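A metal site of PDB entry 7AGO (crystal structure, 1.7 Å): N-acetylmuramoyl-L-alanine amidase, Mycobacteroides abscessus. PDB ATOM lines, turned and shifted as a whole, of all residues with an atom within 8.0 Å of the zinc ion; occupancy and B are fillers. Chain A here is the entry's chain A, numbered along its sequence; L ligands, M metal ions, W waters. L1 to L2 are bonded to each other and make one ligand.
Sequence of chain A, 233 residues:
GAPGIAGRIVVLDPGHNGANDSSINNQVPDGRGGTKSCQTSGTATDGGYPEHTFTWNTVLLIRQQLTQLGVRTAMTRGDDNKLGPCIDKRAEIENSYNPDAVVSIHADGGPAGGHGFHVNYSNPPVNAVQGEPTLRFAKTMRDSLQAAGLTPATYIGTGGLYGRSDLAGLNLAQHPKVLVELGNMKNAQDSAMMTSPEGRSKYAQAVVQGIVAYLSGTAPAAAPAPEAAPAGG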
ATOM      1  N   PRO A  14      23.327  12.534 -25.723  1.00  0.00           N
ATOM      2  CA  PRO A  14      22.255  11.798 -26.401  1.00  0.00           C
ATOM      3  C   PRO A  14      21.246  11.317 -25.374  1.00  0.00           C
ATOM      4  O   PRO A  14      21.543  10.462 -24.533  1.00  0.00           O
ATOM      5  CB  PRO A  14      23.006  10.629 -27.059  1.00  0.00           C
ATOM      6  CG  PRO A  14      24.333  10.505 -26.346  1.00  0.00           C
ATOM      7  CD  PRO A  14      24.490  11.687 -25.414  1.00  0.00           C
ATOM      8  N   GLY A  15      20.032  11.881 -25.441  1.00  0.00           N
ATOM      9  CA  GLY A  15      19.066  11.667 -24.379  1.00  0.00           C
ATOM     10  C   GLY A  15      18.684  10.214 -24.205  1.00  0.00           C
ATOM     11  O   GLY A  15      18.638   9.439 -25.160  1.00  0.00           O
ATOM     12  N   HIS A  16      18.401   9.852 -22.949  1.00  0.00           N
ATOM     13  CA  HIS A  16      17.934   8.542 -22.499  1.00  0.00           C
ATOM     14  C   HIS A  16      19.027   7.476 -22.568  1.00  0.00           C
ATOM     15  O   HIS A  16      20.157   7.754 -22.995  1.00  0.00           O
ATOM     16  CB  HIS A  16      16.687   8.117 -23.271  1.00  0.00           C
ATOM     17  CG  HIS A  16      15.647   9.191 -23.310  1.00  0.00           C
ATOM     18  ND1 HIS A  16      14.824   9.484 -22.239  1.00  0.00           N
ATOM     19  CD2 HIS A  16      15.347  10.094 -24.272  1.00  0.00           C
ATOM     20  CE1 HIS A  16      14.048  10.504 -22.558  1.00  0.00           C
ATOM     21  NE2 HIS A  16      14.331  10.883 -23.785  1.00  0.00           N
ATOM     22  N   GLN A  39      15.673   8.798 -14.670  1.00  0.00           N
ATOM     23  CA  GLN A  39      15.603   8.714 -16.120  1.00  0.00           C
ATOM     24  C   GLN A  39      14.190   8.336 -16.531  1.00  0.00           C
ATOM     25  O   GLN A  39      13.362   7.920 -15.720  1.00  0.00           O
ATOM     26  CB  GLN A  39      16.586   7.668 -16.690  1.00  0.00           C
ATOM     27  CG  GLN A  39      17.915   8.205 -17.216  1.00  0.00           C
ATOM     28  CD  GLN A  39      17.785   9.226 -18.346  1.00  0.00           C
ATOM     29  OE1 GLN A  39      16.713   9.423 -18.926  1.00  0.00           O
ATOM     30  NE2 GLN A  39      18.897   9.887 -18.658  1.00  0.00           N
ATOM     31  N   THR A  40      13.926   8.492 -17.828  1.00  0.00           N
ATOM     32  CA  THR A  40      12.748   7.941 -18.488  1.00  0.00           C
ATOM     33  C   THR A  40      13.205   7.203 -19.733  1.00  0.00           C
ATOM     34  O   THR A  40      14.296   7.464 -20.257  1.00  0.00           O
ATOM     35  CB  THR A  40      11.745   9.034 -18.879  1.00  0.00           C
ATOM     36  OG1 THR A  40      12.375   9.927 -19.785  1.00  0.00           O
ATOM     37  CG2 THR A  40      11.243   9.794 -17.652  1.00  0.00           C
ATOM     38  N   SER A  41      12.377   6.280 -20.212  1.00  0.00           N
ATOM     39  CA  SER A  41      12.803   5.450 -21.333  1.00  0.00           C
ATOM     40  C   SER A  41      12.953   6.246 -22.635  1.00  0.00           C
ATOM     41  O   SER A  41      13.768   5.886 -23.487  1.00  0.00           O
ATOM     42  CB  SER A  41      11.821   4.301 -21.550  1.00  0.00           C
ATOM     43  OG  SER A  41      10.568   4.812 -21.962  1.00  0.00           O
ATOM     44  N   GLY A  42      12.177   7.321 -22.797  1.00  0.00           N
ATOM     45  CA  GLY A  42      12.084   7.992 -24.074  1.00  0.00           C
ATOM     46  C   GLY A  42      11.050   7.331 -24.976  1.00  0.00           C
ATOM     47  O   GLY A  42      10.479   6.296 -24.662  1.00  0.00           O
ATOM     48  N   THR A  43      10.804   7.964 -26.119  1.00  0.00           N
ATOM     49  CA  THR A  43       9.732   7.487 -26.974  1.00  0.00           C
ATOM     50  C   THR A  43      10.316   6.646 -28.122  1.00  0.00           C
ATOM     51  O   THR A  43      11.433   6.126 -28.022  1.00  0.00           O
ATOM     52  CB  THR A  43       8.889   8.697 -27.434  1.00  0.00           C
ATOM     53  OG1 THR A  43       7.738   8.255 -28.161  1.00  0.00           O
ATOM     54  CG2 THR A  43       9.707   9.638 -28.313  1.00  0.00           C
ATOM     55  N   GLU A  51      13.759   6.366 -29.497  1.00  0.00           N
ATOM     56  CA  GLU A  51      14.379   7.671 -29.285  1.00  0.00           C
ATOM     57  C   GLU A  51      15.841   7.526 -28.872  1.00  0.00           C
ATOM     58  O   GLU A  51      16.713   8.223 -29.393  1.00  0.00           O
ATOM     59  CB  GLU A  51      13.615   8.481 -28.233  1.00  0.00           C
ATOM     60  CG  GLU A  51      14.215   9.870 -28.052  1.00  0.00           C
ATOM     61  CD  GLU A  51      13.604  10.679 -26.921  1.00  0.00           C
ATOM     62  OE1 GLU A  51      14.147  11.776 -26.626  1.00  0.00           O
ATOM     63  OE2 GLU A  51      12.574  10.260 -26.364  1.00  0.00           O
ATOM     64  N   HIS A  52      16.137   6.595 -27.946  1.00  0.00           N
ATOM     65  CA  HIS A  52      17.501   6.506 -27.435  1.00  0.00           C
ATOM     66  C   HIS A  52      18.479   6.103 -28.521  1.00  0.00           C
ATOM     67  O   HIS A  52      19.664   6.483 -28.473  1.00  0.00           O
ATOM     68  CB  HIS A  52      17.575   5.554 -26.240  1.00  0.00           C
ATOM     69  CG  HIS A  52      17.270   4.118 -26.570  1.00  0.00           C
ATOM     70  ND1 HIS A  52      18.218   3.243 -27.050  1.00  0.00           N
ATOM     71  CD2 HIS A  52      16.129   3.399 -26.446  1.00  0.00           C
ATOM     72  CE1 HIS A  52      17.668   2.052 -27.218  1.00  0.00           C
ATOM     73  NE2 HIS A  52      16.402   2.115 -26.860  1.00  0.00           N
ATOM     74  N   THR A  55      18.933   9.420 -30.765  1.00  0.00           N
ATOM     75  CA  THR A  55      19.777  10.438 -30.171  1.00  0.00           C
ATOM     76  C   THR A  55      21.222   9.982 -30.152  1.00  0.00           C
ATOM     77  O   THR A  55      22.136  10.770 -30.448  1.00  0.00           O
ATOM     78  CB  THR A  55      19.320  10.772 -28.751  1.00  0.00           C
ATOM     79  OG1 THR A  55      19.464   9.615 -27.919  1.00  0.00           O
ATOM     80  CG2 THR A  55      17.856  11.235 -28.743  1.00  0.00           C
ATOM     81  N   SER A 104      22.123  18.921 -25.618  1.00  0.00           N
ATOM     82  CA  SER A 104      21.392  17.691 -25.371  1.00  0.00           C
ATOM     83  C   SER A 104      20.459  17.435 -26.552  1.00  0.00           C
ATOM     84  O   SER A 104      19.805  18.352 -27.044  1.00  0.00           O
ATOM     85  CB  SER A 104      20.591  17.797 -24.071  1.00  0.00           C
ATOM     86  OG  SER A 104      19.870  16.606 -23.794  1.00  0.00           O
ATOM     87  N   ILE A 105      20.414  16.176 -27.018  1.00  0.00           N
ATOM     88  CA  ILE A 105      19.656  15.815 -28.204  1.00  0.00           C
ATOM     89  C   ILE A 105      18.544  14.850 -27.808  1.00  0.00           C
ATOM     90  O   ILE A 105      18.809  13.806 -27.198  1.00  0.00           O
ATOM     91  CB  ILE A 105      20.555  15.182 -29.291  1.00  0.00           C
ATOM     92  CG1 ILE A 105      21.580  16.199 -29.788  1.00  0.00           C
ATOM     93  CG2 ILE A 105      19.707  14.644 -30.430  1.00  0.00           C
ATOM     94  CD1 ILE A 105      20.961  17.452 -30.431  1.00  0.00           C
ATOM     95  N   HIS A 106      17.312  15.195 -28.190  1.00  0.00           N
ATOM     96  CA  HIS A 106      16.145  14.389 -27.898  1.00  0.00           C
ATOM     97  C   HIS A 106      15.277  14.320 -29.150  1.00  0.00           C
ATOM     98  O   HIS A 106      15.496  15.056 -30.118  1.00  0.00           O
ATOM     99  CB  HIS A 106      15.337  14.987 -26.724  1.00  0.00           C
ATOM    100  CG  HIS A 106      15.911  14.698 -25.369  1.00  0.00           C
ATOM    101  ND1 HIS A 106      15.311  13.837 -24.488  1.00  0.00           N
ATOM    102  CD2 HIS A 106      17.028  15.157 -24.751  1.00  0.00           C
ATOM    103  CE1 HIS A 106      16.036  13.756 -23.379  1.00  0.00           C
ATOM    104  NE2 HIS A 106      17.087  14.554 -23.512  1.00  0.00           N
ATOM    105  N   ALA A 107      14.297  13.434 -29.131  1.00  0.00           N
ATOM    106  CA  ALA A 107      13.194  13.467 -30.085  1.00  0.00           C
ATOM    107  C   ALA A 107      11.898  13.260 -29.319  1.00  0.00           C
ATOM    108  O   ALA A 107      11.878  12.588 -28.273  1.00  0.00           O
ATOM    109  CB  ALA A 107      13.329  12.414 -31.194  1.00  0.00           C
ATOM    110  N   ASP A 108      10.818  13.811 -29.841  1.00  0.00           N
ATOM    111  CA  ASP A 108       9.619  14.069 -29.056  1.00  0.00           C
ATOM    112  C   ASP A 108       8.507  13.100 -29.427  1.00  0.00           C
ATOM    113  O   ASP A 108       8.573  12.401 -30.441  1.00  0.00           O
ATOM    114  CB  ASP A 108       9.177  15.528 -29.289  1.00  0.00           C
ATOM    115  CG  ASP A 108       8.236  16.055 -28.221  1.00  0.00           C
ATOM    116  OD1 ASP A 108       8.155  15.499 -27.110  1.00  0.00           O
ATOM    117  OD2 ASP A 108       7.573  17.057 -28.529  1.00  0.00           O
ATOM    118  N   GLY A 109       7.482  13.071 -28.569  1.00  0.00           N
ATOM    119  CA  GLY A 109       6.240  12.388 -28.881  1.00  0.00           C
ATOM    120  C   GLY A 109       5.083  13.362 -28.811  1.00  0.00           C
ATOM    121  O   GLY A 109       4.738  13.846 -27.727  1.00  0.00           O
ATOM    122  N   LEU A 179      18.623  22.043 -24.971  1.00  0.00           N
ATOM    123  CA  LEU A 179      18.123  20.697 -25.235  1.00  0.00           C
ATOM    124  C   LEU A 179      17.289  20.798 -26.503  1.00  0.00           C
ATOM    125  O   LEU A 179      16.224  21.432 -26.498  1.00  0.00           O
ATOM    126  CB  LEU A 179      17.308  20.151 -24.061  1.00  0.00           C
ATOM    127  CG  LEU A 179      16.888  18.675 -24.069  1.00  0.00           C
ATOM    128  CD1 LEU A 179      16.424  18.221 -22.675  1.00  0.00           C
ATOM    129  CD2 LEU A 179      15.783  18.413 -25.096  1.00  0.00           C
ATOM    130  N   VAL A 180      17.764  20.183 -27.583  1.00  0.00           N
ATOM    131  CA  VAL A 180      17.103  20.266 -28.877  1.00  0.00           C
ATOM    132  C   VAL A 180      16.267  19.014 -29.059  1.00  0.00           C
ATOM    133  O   VAL A 180      16.796  17.905 -29.106  1.00  0.00           O
ATOM    134  CB  VAL A 180      18.115  20.413 -30.026  1.00  0.00           C
ATOM    135  CG1 VAL A 180      17.387  20.562 -31.348  1.00  0.00           C
ATOM    136  CG2 VAL A 180      19.020  21.616 -29.802  1.00  0.00           C
ATOM    137  N   GLU A 181      14.941  19.201 -29.132  1.00  0.00           N
ATOM    138  CA  GLU A 181      14.025  18.166 -29.591  1.00  0.00           C
ATOM    139  C   GLU A 181      13.952  18.286 -31.111  1.00  0.00           C
ATOM    140  O   GLU A 181      13.398  19.257 -31.636  1.00  0.00           O
ATOM    141  CB  GLU A 181      12.647  18.359 -28.958  1.00  0.00           C
ATOM    142  CG  GLU A 181      12.584  18.090 -27.446  1.00  0.00           C
ATOM    143  CD  GLU A 181      12.436  16.626 -27.135  1.00  0.00           C
ATOM    144  OE1 GLU A 181      12.437  15.829 -28.099  1.00  0.00           O
ATOM    145  OE2 GLU A 181      12.314  16.253 -25.934  1.00  0.00           O
ATOM    146  N   MET A 185       8.657  11.985 -33.156  1.00  0.00           N
ATOM    147  CA  MET A 185       8.796  10.624 -33.641  1.00  0.00           C
ATOM    148  C   MET A 185       7.464  10.023 -34.082  1.00  0.00           C
ATOM    149  O   MET A 185       7.460   9.031 -34.841  1.00  0.00           O
ATOM    150  CB  MET A 185       9.407   9.720 -32.563  1.00  0.00           C
ATOM    151  CG  MET A 185      10.738  10.220 -32.017  1.00  0.00           C
ATOM    152  SD  MET A 185      11.715   8.914 -31.225  1.00  0.00           S
ATOM    153  CE  MET A 185      12.746   8.389 -32.611  1.00  0.00           C
HETATM  154  C1  LIG L   1      14.319  12.697 -19.363  1.00  0.00           C
HETATM  155  N1  LIG L   1      12.985  14.307 -20.679  1.00  0.00           N
HETATM  156  O1  LIG L   1      15.088  12.606 -20.325  1.00  0.00           O
HETATM  157  N2  LIG L   1      14.382  11.911 -18.296  1.00  0.00           N
HETATM  158  C2  LIG L   1      13.228  13.746 -19.336  1.00  0.00           C
HETATM  159  C3  LIG L   1      13.559  14.819 -18.288  1.00  0.00           C
HETATM  160  C4  LIG L   1      15.351  16.497 -17.526  1.00  0.00           C
HETATM  161  C5  LIG L   1      14.924  15.446 -18.534  1.00  0.00           C
HETATM  162  O2  LIG L   1      14.568  16.806 -16.592  1.00  0.00           O
HETATM  163  O3  LIG L   1      16.475  17.004 -17.675  1.00  0.00           O
HETATM  164  N1  LG2 L   2      10.424  16.010 -22.634  1.00  0.00           N
HETATM  165  C1  LG2 L   2      11.795  15.582 -22.373  1.00  0.00           C
HETATM  166  C2  LG2 L   2      11.955  15.110 -20.925  1.00  0.00           C
HETATM  167  O1  LG2 L   2      11.107  15.427 -20.083  1.00  0.00           O
HETATM  168  C3  LG2 L   2      12.780  16.699 -22.688  1.00  0.00           C
HETATM  169 ZN    ZN M   1      13.669  12.553 -24.821  1.00  0.00          ZN
HETATM  170  O   HOH W   1      12.079  13.614 -25.703  1.00  0.00           O
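OE2 of Glu 181 is in salt-bridge range of N1 of LG2 L2.
The side-chain hydroxyl (OG1) of Thr 40 is in hydrogen-bond range of a nitrogen (N2) of LIG L1, 3.2 Å away.
OE1 of Gln 39 lies within hydrogen-bond range of N2 of LIG L1, at 3.5 Å.
The side-chain carboxylate of Glu 51 lies close to the backbone NH of Ala 107 (3.0 Å).
The backbone NH of Glu 51 lies within hydrogen-bond range of the backbone carbonyl oxygen of Thr 43, 2.8 Å away.
The side-chain sulfur (SD) of Met 185 lies close to the backbone NH (N) of Glu 51 (3.7 Å).
ND1 of His 16 sits at hydrogen-bond distance from N of Gly 42, 3.5 Å away.
ND1 of His 16 lies within hydrogen-bond range of O of Thr 40 (2.9 Å).
The side-chain hydroxyl of Ser 104 lies close to a ring nitrogen (NE2) of His 106, 3.5 Å away.
N of His 106 lies within hydrogen-bond range of O of Val 180 (2.9 Å).
N of Ala 107 lies close to OE1 of Glu 181 (3.2 Å).
Merely in contact with the zinc ion: Ala 107 (3.9 Å).
Of the 21 residues printed, 4 come within 4 Å of the zinc ion.
The nearest printed residue that does not touch the zinc ion is Glu 181 (4.1 Å).
The zinc ion is bound by the side-chain carboxylate (OE1) of Glu 51 (2.0 Å), a ring nitrogen (NE2) of His 16 (2.1 Å), water W1 (2.1 Å) and a ring nitrogen (ND1) of His 106 (2.1 Å).
The zinc ion has four donor atoms within binding distance.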
